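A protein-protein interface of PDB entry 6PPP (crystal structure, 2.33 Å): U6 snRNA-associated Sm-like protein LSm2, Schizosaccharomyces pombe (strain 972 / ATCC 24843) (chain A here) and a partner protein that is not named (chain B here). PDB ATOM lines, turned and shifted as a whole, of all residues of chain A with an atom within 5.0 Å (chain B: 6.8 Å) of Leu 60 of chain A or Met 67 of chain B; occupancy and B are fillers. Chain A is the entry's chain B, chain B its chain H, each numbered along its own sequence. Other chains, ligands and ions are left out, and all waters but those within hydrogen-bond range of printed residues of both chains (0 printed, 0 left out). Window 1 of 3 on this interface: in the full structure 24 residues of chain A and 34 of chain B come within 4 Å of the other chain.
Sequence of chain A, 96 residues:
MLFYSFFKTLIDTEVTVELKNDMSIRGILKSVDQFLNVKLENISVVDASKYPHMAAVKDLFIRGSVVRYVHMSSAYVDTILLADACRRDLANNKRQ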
ATOM      1  N   LEU A  19      14.089  24.658  -9.633  1.00  0.00           N
ATOM      2  CA  LEU A  19      14.044  25.469  -8.430  1.00  0.00           C
ATOM      3  C   LEU A  19      15.383  26.115  -8.109  1.00  0.00           C
ATOM      4  O   LEU A  19      16.433  25.735  -8.635  1.00  0.00           O
ATOM      5  CB  LEU A  19      13.609  24.608  -7.252  1.00  0.00           C
ATOM      6  CG  LEU A  19      12.196  24.090  -7.208  1.00  0.00           C
ATOM      7  CD1 LEU A  19      12.049  23.021  -8.227  1.00  0.00           C
ATOM      8  CD2 LEU A  19      11.796  23.550  -5.807  1.00  0.00           C
ATOM      9  N   ASN A  21      17.046  25.648  -5.654  1.00  0.00           N
ATOM     10  CA  ASN A  21      17.960  24.686  -5.054  1.00  0.00           C
ATOM     11  C   ASN A  21      18.464  23.644  -6.070  1.00  0.00           C
ATOM     12  O   ASN A  21      18.929  22.560  -5.685  1.00  0.00           O
ATOM     13  CB  ASN A  21      17.320  24.077  -3.794  1.00  0.00           C
ATOM     14  CG  ASN A  21      16.282  22.966  -4.087  1.00  0.00           C
ATOM     15  OD1 ASN A  21      16.487  22.109  -4.962  1.00  0.00           O
ATOM     16  ND2 ASN A  21      15.178  22.965  -3.320  1.00  0.00           N
ATOM     17  N   MET A  23      17.090  21.465  -7.975  1.00  0.00           N
ATOM     18  CA  MET A  23      16.149  20.403  -8.331  1.00  0.00           C
ATOM     19  C   MET A  23      15.232  20.872  -9.453  1.00  0.00           C
ATOM     20  O   MET A  23      14.908  22.063  -9.562  1.00  0.00           O
ATOM     21  CB  MET A  23      15.222  20.033  -7.158  1.00  0.00           C
ATOM     22  CG  MET A  23      15.944  19.390  -5.990  1.00  0.00           C
ATOM     23  SD  MET A  23      14.855  19.167  -4.564  1.00  0.00           S
ATOM     24  CE  MET A  23      13.537  18.234  -5.385  1.00  0.00           C
ATOM     25  N   ILE A  25      11.467  19.602 -11.185  1.00  0.00           N
ATOM     26  CA  ILE A  25      10.336  18.715 -10.928  1.00  0.00           C
ATOM     27  C   ILE A  25       9.369  18.780 -12.101  1.00  0.00           C
ATOM     28  O   ILE A  25       8.900  19.868 -12.465  1.00  0.00           O
ATOM     29  CB  ILE A  25       9.629  19.123  -9.633  1.00  0.00           C
ATOM     30  CG1 ILE A  25      10.617  18.915  -8.463  1.00  0.00           C
ATOM     31  CG2 ILE A  25       8.348  18.326  -9.499  1.00  0.00           C
ATOM     32  CD1 ILE A  25      10.530  19.965  -7.291  1.00  0.00           C
ATOM     33  N   VAL A  38       2.717  27.386  -7.403  1.00  0.00           N
ATOM     34  CA  VAL A  38       2.302  26.485  -8.469  1.00  0.00           C
ATOM     35  C   VAL A  38       2.011  25.089  -7.894  1.00  0.00           C
ATOM     36  O   VAL A  38       2.784  24.558  -7.082  1.00  0.00           O
ATOM     37  CB  VAL A  38       3.425  26.492  -9.519  1.00  0.00           C
ATOM     38  CG1 VAL A  38       4.536  25.603  -9.066  1.00  0.00           C
ATOM     39  CG2 VAL A  38       2.929  26.081 -10.832  1.00  0.00           C
ATOM     40  N   LYS A  39       0.972  24.426  -8.394  1.00  0.00           N
ATOM     41  CA  LYS A  39       0.689  23.045  -7.982  1.00  0.00           C
ATOM     42  C   LYS A  39       0.810  22.104  -9.154  1.00  0.00           C
ATOM     43  O   LYS A  39       0.156  22.312 -10.181  1.00  0.00           O
ATOM     44  CB  LYS A  39      -0.695  22.850  -7.373  1.00  0.00           C
ATOM     45  CG  LYS A  39      -0.901  21.373  -6.972  1.00  0.00           C
ATOM     46  CD  LYS A  39      -2.118  21.153  -6.007  1.00  0.00           C
ATOM     47  CE  LYS A  39      -2.680  19.704  -6.114  1.00  0.00           C
ATOM     48  NZ  LYS A  39      -4.189  19.737  -6.060  1.00  0.00           N
ATOM     49  N   LEU A  40       1.616  21.075  -8.993  1.00  0.00           N
ATOM     50  CA  LEU A  40       1.852  20.076 -10.017  1.00  0.00           C
ATOM     51  C   LEU A  40       1.251  18.753  -9.545  1.00  0.00           C
ATOM     52  O   LEU A  40       1.257  18.438  -8.354  1.00  0.00           O
ATOM     53  CB  LEU A  40       3.355  19.923 -10.290  1.00  0.00           C
ATOM     54  CG  LEU A  40       4.355  21.083 -10.602  1.00  0.00           C
ATOM     55  CD1 LEU A  40       5.764  20.688 -10.298  1.00  0.00           C
ATOM     56  CD2 LEU A  40       4.378  21.488 -12.039  1.00  0.00           C
ATOM     57  N   ILE A  43       3.915  14.271 -10.087  1.00  0.00           N
ATOM     58  CA  ILE A  43       5.271  14.743 -10.337  1.00  0.00           C
ATOM     59  C   ILE A  43       6.184  13.535 -10.447  1.00  0.00           C
ATOM     60  O   ILE A  43       5.863  12.437  -9.974  1.00  0.00           O
ATOM     61  CB  ILE A  43       5.839  15.706  -9.263  1.00  0.00           C
ATOM     62  CG1 ILE A  43       5.965  15.054  -7.899  1.00  0.00           C
ATOM     63  CG2 ILE A  43       5.030  16.990  -9.117  1.00  0.00           C
ATOM     64  CD1 ILE A  43       7.267  14.386  -7.698  1.00  0.00           C
ATOM     65  N   MET A  54      11.093  12.113  -2.471  1.00  0.00           N
ATOM     66  CA  MET A  54       9.756  12.395  -2.941  1.00  0.00           C
ATOM     67  C   MET A  54       9.208  11.184  -3.664  1.00  0.00           C
ATOM     68  O   MET A  54       8.332  11.305  -4.527  1.00  0.00           O
ATOM     69  CB  MET A  54       9.789  13.624  -3.841  1.00  0.00           C
ATOM     70  CG  MET A  54      10.478  14.804  -3.165  1.00  0.00           C
ATOM     71  SD  MET A  54       9.407  16.233  -3.414  1.00  0.00           S
ATOM     72  CE  MET A  54       8.257  16.058  -2.041  1.00  0.00           C
ATOM     73  N   VAL A  57       5.431  10.981  -3.151  1.00  0.00           N
ATOM     74  CA  VAL A  57       4.642  12.183  -3.408  1.00  0.00           C
ATOM     75  C   VAL A  57       4.202  12.188  -4.866  1.00  0.00           C
ATOM     76  O   VAL A  57       5.040  12.214  -5.781  1.00  0.00           O
ATOM     77  CB  VAL A  57       5.469  13.437  -3.084  1.00  0.00           C
ATOM     78  CG1 VAL A  57       4.951  14.641  -3.824  1.00  0.00           C
ATOM     79  CG2 VAL A  57       5.464  13.687  -1.607  1.00  0.00           C
ATOM     80  N   LYS A  58       2.888  12.288  -5.070  1.00  0.00           N
ATOM     81  CA  LYS A  58       2.287  12.483  -6.384  1.00  0.00           C
ATOM     82  C   LYS A  58       1.776  13.901  -6.589  1.00  0.00           C
ATOM     83  O   LYS A  58       1.915  14.439  -7.692  1.00  0.00           O
ATOM     84  CB  LYS A  58       1.145  11.473  -6.621  1.00  0.00           C
ATOM     85  N   ASP A  59       1.168  14.533  -5.588  1.00  0.00           N
ATOM     86  CA  ASP A  59       0.713  15.909  -5.760  1.00  0.00           C
ATOM     87  C   ASP A  59       1.635  16.823  -4.954  1.00  0.00           C
ATOM     88  O   ASP A  59       1.979  16.520  -3.808  1.00  0.00           O
ATOM     89  CB  ASP A  59      -0.736  16.071  -5.301  1.00  0.00           C
ATOM     90  CG  ASP A  59      -1.708  15.398  -6.233  1.00  0.00           C
ATOM     91  OD1 ASP A  59      -1.216  14.602  -7.076  1.00  0.00           O
ATOM     92  OD2 ASP A  59      -2.938  15.682  -6.137  1.00  0.00           O
ATOM     93  N   LEU A  60       2.020  17.951  -5.547  1.00  0.00           N
ATOM     94  CA  LEU A  60       3.125  18.746  -5.021  1.00  0.00           C
ATOM     95  C   LEU A  60       2.859  20.239  -5.202  1.00  0.00           C
ATOM     96  O   LEU A  60       2.477  20.685  -6.287  1.00  0.00           O
ATOM     97  CB  LEU A  60       4.416  18.325  -5.675  1.00  0.00           C
ATOM     98  CG  LEU A  60       5.568  19.232  -5.352  1.00  0.00           C
ATOM     99  CD1 LEU A  60       6.037  18.916  -3.937  1.00  0.00           C
ATOM    100  CD2 LEU A  60       6.660  18.996  -6.413  1.00  0.00           C
ATOM    101  N   PHE A  61       3.029  21.002  -4.133  1.00  0.00           N
ATOM    102  CA  PHE A  61       3.012  22.462  -4.156  1.00  0.00           C
ATOM    103  C   PHE A  61       4.430  23.003  -4.147  1.00  0.00           C
ATOM    104  O   PHE A  61       5.248  22.552  -3.342  1.00  0.00           O
ATOM    105  CB  PHE A  61       2.222  22.961  -2.948  1.00  0.00           C
ATOM    106  CG  PHE A  61       2.317  24.448  -2.682  1.00  0.00           C
ATOM    107  CD1 PHE A  61       3.469  25.030  -2.152  1.00  0.00           C
ATOM    108  CD2 PHE A  61       1.212  25.247  -2.862  1.00  0.00           C
ATOM    109  CE1 PHE A  61       3.514  26.393  -1.869  1.00  0.00           C
ATOM    110  CE2 PHE A  61       1.253  26.613  -2.582  1.00  0.00           C
ATOM    111  CZ  PHE A  61       2.377  27.186  -2.082  1.00  0.00           C
ATOM    112  N   ILE A  62       4.728  23.945  -5.049  1.00  0.00           N
ATOM    113  CA  ILE A  62       6.033  24.609  -5.143  1.00  0.00           C
ATOM    114  C   ILE A  62       5.789  26.089  -4.904  1.00  0.00           C
ATOM    115  O   ILE A  62       4.957  26.695  -5.595  1.00  0.00           O
ATOM    116  CB  ILE A  62       6.687  24.400  -6.510  1.00  0.00           C
ATOM    117  CG1 ILE A  62       6.604  22.908  -6.916  1.00  0.00           C
ATOM    118  CG2 ILE A  62       8.111  24.996  -6.501  1.00  0.00           C
ATOM    119  CD1 ILE A  62       7.488  22.588  -8.137  1.00  0.00           C
ATOM    120  N   ARG A  63       6.539  26.682  -3.978  1.00  0.00           N
ATOM    121  CA  ARG A  63       6.354  28.101  -3.657  1.00  0.00           C
ATOM    122  C   ARG A  63       6.903  28.994  -4.765  1.00  0.00           C
ATOM    123  O   ARG A  63       7.943  28.703  -5.354  1.00  0.00           O
ATOM    124  CB  ARG A  63       7.049  28.448  -2.346  1.00  0.00           C
ATOM    125  CG  ARG A  63       6.554  29.727  -1.656  1.00  0.00           C
ATOM    126  CD  ARG A  63       7.484  30.042  -0.469  1.00  0.00           C
ATOM    127  NE  ARG A  63       6.930  30.966   0.521  1.00  0.00           N
ATOM    128  CZ  ARG A  63       7.436  32.173   0.752  1.00  0.00           C
ATOM    129  NH1 ARG A  63       6.894  32.959   1.682  1.00  0.00           N
ATOM    130  NH2 ARG A  63       8.487  32.600   0.040  1.00  0.00           N
ATOM    131  N   PHE B   6      -4.498  20.095   0.558  1.00  0.00           N
ATOM    132  CA  PHE B   6      -3.727  19.189   1.410  1.00  0.00           C
ATOM    133  C   PHE B   6      -4.199  19.166   2.868  1.00  0.00           C
ATOM    134  O   PHE B   6      -3.656  18.396   3.667  1.00  0.00           O
ATOM    135  CB  PHE B   6      -2.229  19.551   1.376  1.00  0.00           C
ATOM    136  CG  PHE B   6      -1.593  19.456   0.008  1.00  0.00           C
ATOM    137  CD1 PHE B   6      -2.096  18.601  -0.948  1.00  0.00           C
ATOM    138  CD2 PHE B   6      -0.493  20.240  -0.314  1.00  0.00           C
ATOM    139  CE1 PHE B   6      -1.532  18.535  -2.201  1.00  0.00           C
ATOM    140  CE2 PHE B   6       0.089  20.166  -1.567  1.00  0.00           C
ATOM    141  CZ  PHE B   6      -0.433  19.306  -2.512  1.00  0.00           C
ATOM    142  N   VAL B  11       1.685  15.302   4.793  1.00  0.00           N
ATOM    143  CA  VAL B  11       2.298  16.277   3.922  1.00  0.00           C
ATOM    144  C   VAL B  11       3.790  16.184   4.204  1.00  0.00           C
ATOM    145  O   VAL B  11       4.204  15.821   5.309  1.00  0.00           O
ATOM    146  CB  VAL B  11       1.650  17.651   4.219  1.00  0.00           C
ATOM    147  CG1 VAL B  11       2.552  18.788   3.903  1.00  0.00           C
ATOM    148  CG2 VAL B  11       0.312  17.768   3.488  1.00  0.00           C
ATOM    149  N   GLN B  12       4.597  16.493   3.196  1.00  0.00           N
ATOM    150  CA  GLN B  12       6.049  16.412   3.291  1.00  0.00           C
ATOM    151  C   GLN B  12       6.618  17.744   2.828  1.00  0.00           C
ATOM    152  O   GLN B  12       6.495  18.100   1.650  1.00  0.00           O
ATOM    153  CB  GLN B  12       6.588  15.229   2.458  1.00  0.00           C
ATOM    154  CG  GLN B  12       8.075  15.279   2.103  1.00  0.00           C
ATOM    155  CD  GLN B  12       8.690  13.901   1.847  1.00  0.00           C
ATOM    156  OE1 GLN B  12       8.543  12.969   2.649  1.00  0.00           O
ATOM    157  NE2 GLN B  12       9.431  13.786   0.757  1.00  0.00           N
ATOM    158  N   VAL B  13       7.275  18.454   3.730  1.00  0.00           N
ATOM    159  CA  VAL B  13       7.756  19.788   3.452  1.00  0.00           C
ATOM    160  C   VAL B  13       9.234  19.689   3.176  1.00  0.00           C
ATOM    161  O   VAL B  13       9.970  19.039   3.927  1.00  0.00           O
ATOM    162  CB  VAL B  13       7.472  20.732   4.634  1.00  0.00           C
ATOM    163  CG1 VAL B  13       8.000  22.136   4.362  1.00  0.00           C
ATOM    164  CG2 VAL B  13       5.987  20.754   4.929  1.00  0.00           C
ATOM    165  N   ILE B  14       9.660  20.312   2.092  1.00  0.00           N
ATOM    166  CA  ILE B  14      11.069  20.527   1.796  1.00  0.00           C
ATOM    167  C   ILE B  14      11.284  21.998   2.074  1.00  0.00           C
ATOM    168  O   ILE B  14      10.529  22.844   1.559  1.00  0.00           O
ATOM    169  CB  ILE B  14      11.431  20.188   0.345  1.00  0.00           C
ATOM    170  CG1 ILE B  14      11.010  18.756  -0.016  1.00  0.00           C
ATOM    171  CG2 ILE B  14      12.904  20.430   0.135  1.00  0.00           C
ATOM    172  CD1 ILE B  14      11.905  17.729   0.640  1.00  0.00           C
ATOM    173  N   THR B  15      12.225  22.282   2.955  1.00  0.00           N
ATOM    174  CA  THR B  15      12.521  23.627   3.408  1.00  0.00           C
ATOM    175  C   THR B  15      13.715  24.215   2.682  1.00  0.00           C
ATOM    176  O   THR B  15      14.557  23.494   2.139  1.00  0.00           O
ATOM    177  CB  THR B  15      12.809  23.588   4.907  1.00  0.00           C
ATOM    178  OG1 THR B  15      13.665  22.469   5.191  1.00  0.00           O
ATOM    179  CG2 THR B  15      11.480  23.437   5.644  1.00  0.00           C
ATOM    180  N   ASN B  16      13.896  25.528   2.864  1.00  0.00           N
ATOM    181  CA  ASN B  16      14.962  26.204   2.136  1.00  0.00           C
ATOM    182  C   ASN B  16      16.345  25.763   2.581  1.00  0.00           C
ATOM    183  O   ASN B  16      17.289  25.887   1.790  1.00  0.00           O
ATOM    184  CB  ASN B  16      14.814  27.709   2.313  1.00  0.00           C
ATOM    185  CG  ASN B  16      13.673  28.256   1.511  1.00  0.00           C
ATOM    186  OD1 ASN B  16      13.106  27.543   0.669  1.00  0.00           O
ATOM    187  ND2 ASN B  16      13.326  29.521   1.745  1.00  0.00           N
ATOM    188  N   LEU B  34       3.002  27.353   7.855  1.00  0.00           N
ATOM    189  CA  LEU B  34       2.224  26.124   7.985  1.00  0.00           C
ATOM    190  C   LEU B  34       2.171  25.614   9.430  1.00  0.00           C
ATOM    191  O   LEU B  34       3.160  25.678  10.176  1.00  0.00           O
ATOM    192  CB  LEU B  34       2.799  25.016   7.075  1.00  0.00           C
ATOM    193  CG  LEU B  34       3.217  25.305   5.626  1.00  0.00           C
ATOM    194  CD1 LEU B  34       4.099  24.179   5.135  1.00  0.00           C
ATOM    195  CD2 LEU B  34       2.036  25.433   4.697  1.00  0.00           C
ATOM    196  N   ASN B  64      10.702  30.137   4.411  1.00  0.00           N
ATOM    197  CA  ASN B  64      11.600  28.990   4.420  1.00  0.00           C
ATOM    198  C   ASN B  64      11.043  27.755   3.716  1.00  0.00           C
ATOM    199  O   ASN B  64      11.662  26.688   3.785  1.00  0.00           O
ATOM    200  CB  ASN B  64      12.011  28.621   5.842  1.00  0.00           C
ATOM    201  CG  ASN B  64      13.387  28.004   5.873  1.00  0.00           C
ATOM    202  OD1 ASN B  64      13.539  26.795   6.076  1.00  0.00           O
ATOM    203  ND2 ASN B  64      14.412  28.833   5.632  1.00  0.00           N
ATOM    204  N   VAL B  65       9.862  27.845   3.125  1.00  0.00           N
ATOM    205  CA  VAL B  65       9.202  26.712   2.485  1.00  0.00           C
ATOM    206  C   VAL B  65       9.515  26.688   0.982  1.00  0.00           C
ATOM    207  O   VAL B  65       9.250  27.657   0.265  1.00  0.00           O
ATOM    208  CB  VAL B  65       7.686  26.803   2.722  1.00  0.00           C
ATOM    209  CG1 VAL B  65       6.956  25.539   2.275  1.00  0.00           C
ATOM    210  CG2 VAL B  65       7.410  27.139   4.193  1.00  0.00           C
ATOM    211  N   ALA B  66      10.097  25.586   0.495  1.00  0.00           N
ATOM    212  CA  ALA B  66      10.268  25.413  -0.948  1.00  0.00           C
ATOM    213  C   ALA B  66       9.117  24.595  -1.512  1.00  0.00           C
ATOM    214  O   ALA B  66       8.435  25.051  -2.440  1.00  0.00           O
ATOM    215  CB  ALA B  66      11.600  24.749  -1.300  1.00  0.00           C
ATOM    216  N   MET B  67       8.820  23.428  -0.927  1.00  0.00           N
ATOM    217  CA  MET B  67       7.771  22.565  -1.497  1.00  0.00           C
ATOM    218  C   MET B  67       6.961  21.913  -0.385  1.00  0.00           C
ATOM    219  O   MET B  67       7.479  21.611   0.700  1.00  0.00           O
ATOM    220  CB  MET B  67       8.269  21.435  -2.414  1.00  0.00           C
ATOM    221  CG  MET B  67       9.249  21.833  -3.469  1.00  0.00           C
ATOM    222  SD  MET B  67      10.069  20.309  -3.939  1.00  0.00           S
ATOM    223  CE  MET B  67      11.777  20.748  -3.806  1.00  0.00           C
ATOM    224  N   VAL B  68       5.693  21.662  -0.682  1.00  0.00           N
ATOM    225  CA  VAL B  68       4.803  20.858   0.159  1.00  0.00           C
ATOM    226  C   VAL B  68       4.192  19.745  -0.691  1.00  0.00           C
ATOM    227  O   VAL B  68       3.315  20.011  -1.523  1.00  0.00           O
ATOM    228  CB  VAL B  68       3.706  21.745   0.748  1.00  0.00           C
ATOM    229  CG1 VAL B  68       2.727  20.952   1.580  1.00  0.00           C
ATOM    230  CG2 VAL B  68       4.360  22.909   1.502  1.00  0.00           C
ATOM    231  N   GLY B  69       4.563  18.496  -0.408  1.00  0.00           N
ATOM    232  CA  GLY B  69       4.080  17.347  -1.164  1.00  0.00           C
ATOM    233  C   GLY B  69       3.029  16.572  -0.389  1.00  0.00           C
ATOM    234  O   GLY B  69       3.083  16.489   0.836  1.00  0.00           O
ATOM    235  N   LEU B  70       2.037  16.055  -1.117  1.00  0.00           N
ATOM    236  CA  LEU B  70       0.992  15.205  -0.543  1.00  0.00           C
ATOM    237  C   LEU B  70       1.503  13.773  -0.580  1.00  0.00           C
ATOM    238  O   LEU B  70       1.768  13.246  -1.668  1.00  0.00           O
ATOM    239  CB  LEU B  70      -0.288  15.362  -1.357  1.00  0.00           C
ATOM    240  CG  LEU B  70      -1.579  14.650  -0.965  1.00  0.00           C
ATOM    241  CD1 LEU B  70      -2.105  15.262   0.313  1.00  0.00           C
ATOM    242  CD2 LEU B  70      -2.606  14.760  -2.088  1.00  0.00           C
ATOM    243  N   ILE B  89      19.566  17.299   0.081  1.00  0.00           N
ATOM    244  CA  ILE B  89      18.867  18.322  -0.713  1.00  0.00           C
ATOM    245  C   ILE B  89      19.618  19.648  -0.592  1.00  0.00           C
ATOM    246  O   ILE B  89      19.915  20.087   0.539  1.00  0.00           O
ATOM    247  CB  ILE B  89      17.441  18.462  -0.227  1.00  0.00           C
ATOM    248  CG1 ILE B  89      16.737  17.114  -0.371  1.00  0.00           C
ATOM    249  CG2 ILE B  89      16.730  19.591  -0.973  1.00  0.00           C
ATOM    250  CD1 ILE B  89      15.279  17.173  -0.158  1.00  0.00           C
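Of the 16 printed residues of chain B, 8 touch a printed residue of chain A. Printed residues of chain A that touch a printed residue of chain B: Leu 19, Met 23, Ile 25, Met 54, Val 57, Lys 58, Asp 59, Leu 60, Phe 61, Ile 62 and Arg 63. Hydrophobic or aromatic side chains of chain A within 4 Å of the printed part of chain B: Leu 19, Met 23, Ile 25, Met 54, Val 57, Leu 60 and Phe 61. Among the printed residues, 19 pairs touch across the chains. Among the printed residues, no Asp or Glu carboxylate lies within 4 Å of a Lys or Arg side-chain nitrogen of the other chain.
Printed residues of chain B within 4 Å of Met 23 of chain A: Met 67. Of chain B, only Met 67, Val 68 and Gly 69 come within 4 Å of Leu 60 of chain A. Of the printed residues of chain B, Phe 61 of chain A touches Phe 6 (3.8 Å), Met 67 (3.1 Å) and Val 68 (2.8 Å). Printed residues of chain B within 4 Å of Ile 62 of chain A: Ala 66 (3.6 Å). Of the printed residues of chain A, Val 65 of chain B touches Arg 63 (3.1 Å). Met 67 of chain B touches just these residues of chain A: Leu 19 (3.4 Å), Met 23 (3.5 Å), Ile 25 (3.4 Å), Leu 60 (3.7 Å) and Phe 61 (3.1 Å). Ile 89 of chain B touches none of the printed residues of chain A. The nearest residue of chain B that does not touch Leu 60 of chain A is Phe 6 of chain B (4.1 Å).
The backbone carbonyl oxygen (O) of Asp 59 of chain A lies within hydrogen-bond range of the backbone NH (N) of Leu 70 of chain B, 2.7 Å away. The backbone NH of Phe 61 of chain A is in hydrogen-bond range of the backbone carbonyl oxygen of Val 68 of chain B (2.8 Å). The backbone carbonyl oxygen of Ala 66 of chain B sits at hydrogen-bond distance from the backbone NH of Arg 63 of chain A, at 2.9 Å.
The backbone carbonyl oxygen (O) of Ile 14 of chain B sits at hydrogen-bond distance from the backbone NH (N) of Ala 66 of chain B (3.0 Å). O of Lys 58 of chain A is in hydrogen-bond range of N of Ile 43 of chain A. The backbone carbonyl oxygen (O) of Val 38 of chain A sits at hydrogen-bond distance from the backbone NH (N) of Ile 62 of chain A (2.9 Å). OD1 of Asn 21 of chain A sits close to N of Met 23 of chain A, at 3.1 Å. N of Gln 12 of chain B sits at hydrogen-bond distance from O of Gly 69 of chain B (2.8 Å). The backbone NH (N) of Leu 40 of chain A is in hydrogen-bond range of the backbone carbonyl oxygen (O) of Leu 60 of chain A (2.9 Å).
Leu 19 of chain A touches Met 67 of chain B (CD2 to CE, 3.4 Å). CD1 of Ile 25 of chain A touches SD of Met 67 of chain B, at 3.4 Å. Gln 12 of chain B touches Met 54 of chain A (NE2 to CE, 3.8 Å). Val 57 of chain A touches Gly 69 of chain B. Lys 58 of chain A touches Leu 70 of chain B. O of Asp 59 of chain A touches CA of Gly 69 of chain B (3.5 Å). Leu 60 of chain A touches Gly 69 of chain B (CD1 to CA, 3.7 Å). Phe 61 of chain A touches Phe 6 of chain B. Met 67 of chain B touches Phe 61 of chain A (CA to O, 3.1 Å). Ala 66 of chain B touches Ile 62 of chain A.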
